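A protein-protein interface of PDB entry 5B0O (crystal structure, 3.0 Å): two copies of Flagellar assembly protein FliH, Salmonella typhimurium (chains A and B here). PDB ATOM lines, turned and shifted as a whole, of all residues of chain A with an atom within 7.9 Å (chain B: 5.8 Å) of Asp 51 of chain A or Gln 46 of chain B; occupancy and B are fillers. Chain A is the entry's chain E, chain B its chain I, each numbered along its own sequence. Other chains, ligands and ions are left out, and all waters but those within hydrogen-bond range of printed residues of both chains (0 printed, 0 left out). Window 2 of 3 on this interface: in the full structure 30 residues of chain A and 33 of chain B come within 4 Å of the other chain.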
ATOM      1  N   PRO A  48      16.362  -7.733  32.860  1.00  0.00           N
ATOM      2  CA  PRO A  48      15.483  -7.842  31.691  1.00  0.00           C
ATOM      3  C   PRO A  48      16.141  -8.783  30.692  1.00  0.00           C
ATOM      4  O   PRO A  48      17.284  -9.185  30.910  1.00  0.00           O
ATOM      5  CB  PRO A  48      15.463  -6.416  31.120  1.00  0.00           C
ATOM      6  CG  PRO A  48      16.160  -5.541  32.159  1.00  0.00           C
ATOM      7  CD  PRO A  48      17.109  -6.469  32.867  1.00  0.00           C
ATOM      8  N   ALA A  49      15.457  -9.099  29.600  1.00  0.00           N
ATOM      9  CA  ALA A  49      16.019  -9.976  28.581  1.00  0.00           C
ATOM     10  C   ALA A  49      15.310  -9.745  27.258  1.00  0.00           C
ATOM     11  O   ALA A  49      14.181  -9.252  27.217  1.00  0.00           O
ATOM     12  CB  ALA A  49      15.903 -11.434  29.005  1.00  0.00           C
ATOM     13  N   VAL A  50      15.969 -10.107  26.169  1.00  0.00           N
ATOM     14  CA  VAL A  50      15.452  -9.752  24.859  1.00  0.00           C
ATOM     15  C   VAL A  50      14.599 -10.846  24.221  1.00  0.00           C
ATOM     16  O   VAL A  50      14.125 -10.695  23.091  1.00  0.00           O
ATOM     17  CB  VAL A  50      16.598  -9.403  23.892  1.00  0.00           C
ATOM     18  CG1 VAL A  50      16.537  -7.935  23.499  1.00  0.00           C
ATOM     19  CG2 VAL A  50      17.944  -9.738  24.519  1.00  0.00           C
ATOM     20  N   ASP A  51      14.377 -11.939  24.940  1.00  0.00           N
ATOM     21  CA  ASP A  51      13.542 -12.991  24.375  1.00  0.00           C
ATOM     22  C   ASP A  51      12.096 -12.942  24.852  1.00  0.00           C
ATOM     23  O   ASP A  51      11.792 -13.205  26.016  1.00  0.00           O
ATOM     24  CB  ASP A  51      14.146 -14.378  24.597  1.00  0.00           C
ATOM     25  CG  ASP A  51      15.087 -14.785  23.479  1.00  0.00           C
ATOM     26  OD1 ASP A  51      14.598 -15.210  22.407  1.00  0.00           O
ATOM     27  OD2 ASP A  51      16.318 -14.673  23.669  1.00  0.00           O
ATOM     28  N   ASN A  52      11.210 -12.594  23.925  1.00  0.00           N
ATOM     29  CA  ASN A  52       9.781 -12.689  24.148  1.00  0.00           C
ATOM     30  C   ASN A  52       9.300 -14.067  23.713  1.00  0.00           C
ATOM     31  O   ASN A  52       8.098 -14.330  23.685  1.00  0.00           O
ATOM     32  CB  ASN A  52       9.010 -11.611  23.374  1.00  0.00           C
ATOM     33  CG  ASN A  52       9.901 -10.511  22.825  1.00  0.00           C
ATOM     34  OD1 ASN A  52      10.318  -9.613  23.556  1.00  0.00           O
ATOM     35  ND2 ASN A  52      10.155 -10.550  21.518  1.00  0.00           N
ATOM     36  N   SER A  53      10.243 -14.936  23.363  1.00  0.00           N
ATOM     37  CA  SER A  53       9.921 -16.232  22.787  1.00  0.00           C
ATOM     38  C   SER A  53       8.788 -16.909  23.561  1.00  0.00           C
ATOM     39  O   SER A  53       7.813 -17.370  22.969  1.00  0.00           O
ATOM     40  CB  SER A  53      11.170 -17.117  22.779  1.00  0.00           C
ATOM     41  OG  SER A  53      10.958 -18.318  22.055  1.00  0.00           O
ATOM     42  N   ALA A  54       8.908 -16.939  24.885  1.00  0.00           N
ATOM     43  CA  ALA A  54       7.882 -17.524  25.745  1.00  0.00           C
ATOM     44  C   ALA A  54       6.674 -16.597  25.905  1.00  0.00           C
ATOM     45  O   ALA A  54       5.527 -17.051  25.888  1.00  0.00           O
ATOM     46  CB  ALA A  54       8.468 -17.871  27.104  1.00  0.00           C
ATOM     47  N   LEU A  55       6.938 -15.302  26.078  1.00  0.00           N
ATOM     48  CA  LEU A  55       5.875 -14.304  26.170  1.00  0.00           C
ATOM     49  C   LEU A  55       5.042 -14.281  24.892  1.00  0.00           C
ATOM     50  O   LEU A  55       3.814 -14.296  24.945  1.00  0.00           O
ATOM     51  CB  LEU A  55       6.450 -12.912  26.453  1.00  0.00           C
ATOM     52  CG  LEU A  55       5.470 -11.737  26.395  1.00  0.00           C
ATOM     53  CD1 LEU A  55       4.347 -11.954  27.370  1.00  0.00           C
ATOM     54  CD2 LEU A  55       6.160 -10.418  26.681  1.00  0.00           C
ATOM     55  N   ILE A  56       5.713 -14.259  23.745  1.00  0.00           N
ATOM     56  CA  ILE A  56       5.015 -14.285  22.464  1.00  0.00           C
ATOM     57  C   ILE A  56       4.173 -15.546  22.287  1.00  0.00           C
ATOM     58  O   ILE A  56       3.178 -15.534  21.574  1.00  0.00           O
ATOM     59  CB  ILE A  56       5.983 -14.147  21.278  1.00  0.00           C
ATOM     60  CG1 ILE A  56       6.617 -12.764  21.285  1.00  0.00           C
ATOM     61  CG2 ILE A  56       5.243 -14.341  19.962  1.00  0.00           C
ATOM     62  CD1 ILE A  56       5.601 -11.656  21.184  1.00  0.00           C
ATOM     63  N   ASP A  81       8.929  -4.888  26.641  1.00  0.00           N
ATOM     64  CA  ASP A  81       8.487  -5.964  25.756  1.00  0.00           C
ATOM     65  C   ASP A  81       7.557  -5.404  24.684  1.00  0.00           C
ATOM     66  O   ASP A  81       7.300  -6.054  23.675  1.00  0.00           O
ATOM     67  CB  ASP A  81       7.725  -7.044  26.530  1.00  0.00           C
ATOM     68  CG  ASP A  81       8.610  -7.859  27.451  1.00  0.00           C
ATOM     69  OD1 ASP A  81       9.702  -8.298  27.027  1.00  0.00           O
ATOM     70  OD2 ASP A  81       8.192  -8.071  28.610  1.00  0.00           O
ATOM     71  N   ARG A  84       8.469  -4.787  20.666  1.00  0.00           N
ATOM     72  CA  ARG A  84       8.767  -6.050  20.005  1.00  0.00           C
ATOM     73  C   ARG A  84       7.508  -6.896  19.814  1.00  0.00           C
ATOM     74  O   ARG A  84       7.286  -7.462  18.747  1.00  0.00           O
ATOM     75  CB  ARG A  84       9.837  -6.804  20.796  1.00  0.00           C
ATOM     76  CG  ARG A  84      11.089  -5.962  21.041  1.00  0.00           C
ATOM     77  CD  ARG A  84      12.157  -6.718  21.805  1.00  0.00           C
ATOM     78  NE  ARG A  84      11.980  -6.621  23.250  1.00  0.00           N
ATOM     79  CZ  ARG A  84      12.371  -7.558  24.105  1.00  0.00           C
ATOM     80  NH1 ARG A  84      12.942  -8.662  23.650  1.00  0.00           N
ATOM     81  NH2 ARG A  84      12.180  -7.402  25.408  1.00  0.00           N
ATOM     82  N   HIS A 108       8.987  -8.192  32.782  1.00  0.00           N
ATOM     83  CA  HIS A 108       9.296  -8.720  31.459  1.00  0.00           C
ATOM     84  C   HIS A 108       8.894 -10.187  31.346  1.00  0.00           C
ATOM     85  O   HIS A 108       9.073 -10.950  32.285  1.00  0.00           O
ATOM     86  CB  HIS A 108      10.798  -8.587  31.181  1.00  0.00           C
ATOM     87  CG  HIS A 108      11.328  -7.195  31.335  1.00  0.00           C
ATOM     88  ND1 HIS A 108      11.219  -6.476  32.505  1.00  0.00           N
ATOM     89  CD2 HIS A 108      11.996  -6.398  30.466  1.00  0.00           C
ATOM     90  CE1 HIS A 108      11.785  -5.293  32.349  1.00  0.00           C
ATOM     91  NE2 HIS A 108      12.264  -5.221  31.119  1.00  0.00           N
ATOM     92  N   GLY A 109       8.345 -10.580  30.200  1.00  0.00           N
ATOM     93  CA  GLY A 109       8.045 -11.980  29.944  1.00  0.00           C
ATOM     94  C   GLY A 109       6.678 -12.398  30.445  1.00  0.00           C
ATOM     95  O   GLY A 109       6.372 -13.589  30.528  1.00  0.00           O
ATOM     96  N   GLY A 110       5.845 -11.407  30.750  1.00  0.00           N
ATOM     97  CA  GLY A 110       4.520 -11.638  31.298  1.00  0.00           C
ATOM     98  C   GLY A 110       3.550 -10.549  30.888  1.00  0.00           C
ATOM     99  O   GLY A 110       3.966  -9.449  30.523  1.00  0.00           O
ATOM    100  N   ARG A 127       2.394 -15.478  38.950  1.00  0.00           N
ATOM    101  CA  ARG A 127       3.024 -16.797  38.907  1.00  0.00           C
ATOM    102  C   ARG A 127       3.979 -17.025  40.079  1.00  0.00           C
ATOM    103  O   ARG A 127       4.226 -18.163  40.458  1.00  0.00           O
ATOM    104  CB  ARG A 127       3.774 -17.001  37.600  1.00  0.00           C
ATOM    105  CG  ARG A 127       2.955 -16.748  36.366  1.00  0.00           C
ATOM    106  CD  ARG A 127       3.855 -16.846  35.158  1.00  0.00           C
ATOM    107  NE  ARG A 127       3.126 -16.822  33.900  1.00  0.00           N
ATOM    108  CZ  ARG A 127       3.712 -16.708  32.716  1.00  0.00           C
ATOM    109  NH1 ARG A 127       5.031 -16.598  32.644  1.00  0.00           N
ATOM    110  NH2 ARG A 127       2.984 -16.693  31.608  1.00  0.00           N
ATOM    111  N   ALA B  40      12.917 -19.346  38.789  1.00  0.00           N
ATOM    112  CA  ALA B  40      12.972 -18.235  37.851  1.00  0.00           C
ATOM    113  C   ALA B  40      12.385 -18.665  36.521  1.00  0.00           C
ATOM    114  O   ALA B  40      11.437 -18.064  36.031  1.00  0.00           O
ATOM    115  CB  ALA B  40      14.405 -17.777  37.661  1.00  0.00           C
ATOM    116  N   ARG B  41      12.941 -19.733  35.962  1.00  0.00           N
ATOM    117  CA  ARG B  41      12.499 -20.272  34.679  1.00  0.00           C
ATOM    118  C   ARG B  41      10.995 -20.501  34.579  1.00  0.00           C
ATOM    119  O   ARG B  41      10.349 -20.022  33.652  1.00  0.00           O
ATOM    120  CB  ARG B  41      13.206 -21.596  34.403  1.00  0.00           C
ATOM    121  CG  ARG B  41      12.552 -22.421  33.317  1.00  0.00           C
ATOM    122  CD  ARG B  41      13.162 -23.798  33.232  1.00  0.00           C
ATOM    123  NE  ARG B  41      12.948 -24.387  31.916  1.00  0.00           N
ATOM    124  CZ  ARG B  41      13.611 -25.441  31.453  1.00  0.00           C
ATOM    125  NH1 ARG B  41      14.538 -26.029  32.199  1.00  0.00           N
ATOM    126  NH2 ARG B  41      13.348 -25.903  30.237  1.00  0.00           N
ATOM    127  N   GLN B  42      10.442 -21.252  35.521  1.00  0.00           N
ATOM    128  CA  GLN B  42       9.023 -21.573  35.488  1.00  0.00           C
ATOM    129  C   GLN B  42       8.162 -20.320  35.565  1.00  0.00           C
ATOM    130  O   GLN B  42       7.048 -20.291  35.050  1.00  0.00           O
ATOM    131  CB  GLN B  42       8.660 -22.499  36.646  1.00  0.00           C
ATOM    132  CG  GLN B  42       7.324 -23.182  36.471  1.00  0.00           C
ATOM    133  CD  GLN B  42       7.388 -24.290  35.444  1.00  0.00           C
ATOM    134  OE1 GLN B  42       8.260 -25.159  35.511  1.00  0.00           O
ATOM    135  NE2 GLN B  42       6.471 -24.264  34.482  1.00  0.00           N
ATOM    136  N   ILE B  44       9.165 -17.039  34.616  1.00  0.00           N
ATOM    137  CA  ILE B  44       9.406 -16.199  33.445  1.00  0.00           C
ATOM    138  C   ILE B  44       9.046 -16.898  32.130  1.00  0.00           C
ATOM    139  O   ILE B  44       8.706 -16.251  31.137  1.00  0.00           O
ATOM    140  CB  ILE B  44      10.862 -15.704  33.433  1.00  0.00           C
ATOM    141  CG1 ILE B  44      11.064 -14.710  34.576  1.00  0.00           C
ATOM    142  CG2 ILE B  44      11.210 -15.061  32.112  1.00  0.00           C
ATOM    143  CD1 ILE B  44      12.490 -14.275  34.766  1.00  0.00           C
ATOM    144  N   GLY B  45       9.111 -18.224  32.133  1.00  0.00           N
ATOM    145  CA  GLY B  45       8.693 -18.998  30.981  1.00  0.00           C
ATOM    146  C   GLY B  45       9.848 -19.395  30.090  1.00  0.00           C
ATOM    147  O   GLY B  45       9.661 -20.090  29.089  1.00  0.00           O
ATOM    148  N   GLN B  46      11.045 -18.943  30.452  1.00  0.00           N
ATOM    149  CA  GLN B  46      12.258 -19.341  29.748  1.00  0.00           C
ATOM    150  C   GLN B  46      13.467 -19.247  30.661  1.00  0.00           C
ATOM    151  O   GLN B  46      13.451 -18.517  31.650  1.00  0.00           O
ATOM    152  CB  GLN B  46      12.468 -18.469  28.517  1.00  0.00           C
ATOM    153  CG  GLN B  46      12.534 -16.987  28.810  1.00  0.00           C
ATOM    154  CD  GLN B  46      12.446 -16.159  27.549  1.00  0.00           C
ATOM    155  OE1 GLN B  46      13.451 -15.917  26.883  1.00  0.00           O
ATOM    156  NE2 GLN B  46      11.234 -15.728  27.205  1.00  0.00           N
ATOM    157  N   THR B  47      14.513 -19.994  30.327  1.00  0.00           N
ATOM    158  CA  THR B  47      15.751 -19.957  31.088  1.00  0.00           C
ATOM    159  C   THR B  47      16.397 -18.590  30.951  1.00  0.00           C
ATOM    160  O   THR B  47      16.699 -18.154  29.841  1.00  0.00           O
ATOM    161  CB  THR B  47      16.735 -21.026  30.600  1.00  0.00           C
ATOM    162  OG1 THR B  47      16.122 -22.317  30.704  1.00  0.00           O
ATOM    163  CG2 THR B  47      18.010 -20.998  31.429  1.00  0.00           C
ATOM    164  N   PRO B  48      16.603 -17.899  32.081  1.00  0.00           N
ATOM    165  CA  PRO B  48      17.187 -16.564  31.972  1.00  0.00           C
ATOM    166  C   PRO B  48      18.690 -16.674  31.831  1.00  0.00           C
ATOM    167  O   PRO B  48      19.232 -17.768  31.956  1.00  0.00           O
ATOM    168  CB  PRO B  48      16.835 -15.927  33.318  1.00  0.00           C
ATOM    169  CG  PRO B  48      16.772 -17.080  34.264  1.00  0.00           C
ATOM    170  CD  PRO B  48      16.295 -18.268  33.474  1.00  0.00           C
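The side-chain amide nitrogen of Gln 46 of chain B is in hydrogen-bond range of the backbone carbonyl oxygen of Asp 51 of chain A, 2.8 Å away.
The backbone carbonyl oxygen of Arg 41 of chain B sits at hydrogen-bond distance from the backbone NH of Gln 46 of chain B, at 3.4 Å. The side-chain carboxylate (OD2) of Asp 81 of chain A lies within hydrogen-bond range of the backbone NH (N) of Gly 109 of chain A (3.0 Å).
Ala 54 of chain A touches Gly 45 of chain B. Ala 54 of chain A touches Gln 46 of chain B (CB to NE2, 3.5 Å). O of Gly 109 of chain A touches O of Ile 44 of chain B, 3.6 Å away. O of Ile 44 of chain B touches NH1 of Arg 127 of chain A (3.99 Å).
Of the printed residues of chain B, Asp 51 of chain A touches Gln 46 (2.8 Å). Printed residues of chain B within 4 Å of Ala 54 of chain A: Gly 45 (3.2 Å) and Gln 46 (3.5 Å). Of the printed residues of chain B, Gly 109 of chain A touches Ile 44 (3.6 Å). Of the printed residues of chain B, Arg 127 of chain A touches Ile 44. Printed residues of chain A within 4 Å of Ile 44 of chain B: Gly 109 (3.6 Å) and Arg 127 (3.99 Å). Of chain A, only Ala 54 comes within 4 Å of Gly 45 of chain B. Of chain A, only Asp 51 (2.8 Å) and Ala 54 (3.5 Å) come within 4 Å of Gln 46 of chain B. The nearest printed residue of chain B that does not touch Asp 51 of chain A is Ile 44 of chain B (6.4 Å).
Printed residues of chain B that touch a printed residue of chain A: Ile 44, Gly 45 and Gln 46. Hydrophobic or aromatic side chains of chain A within 4 Å of the printed part of chain B: Ala 54. Among the printed residues, 5 pairs touch across the chains.
Position printed for both chains: 48.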
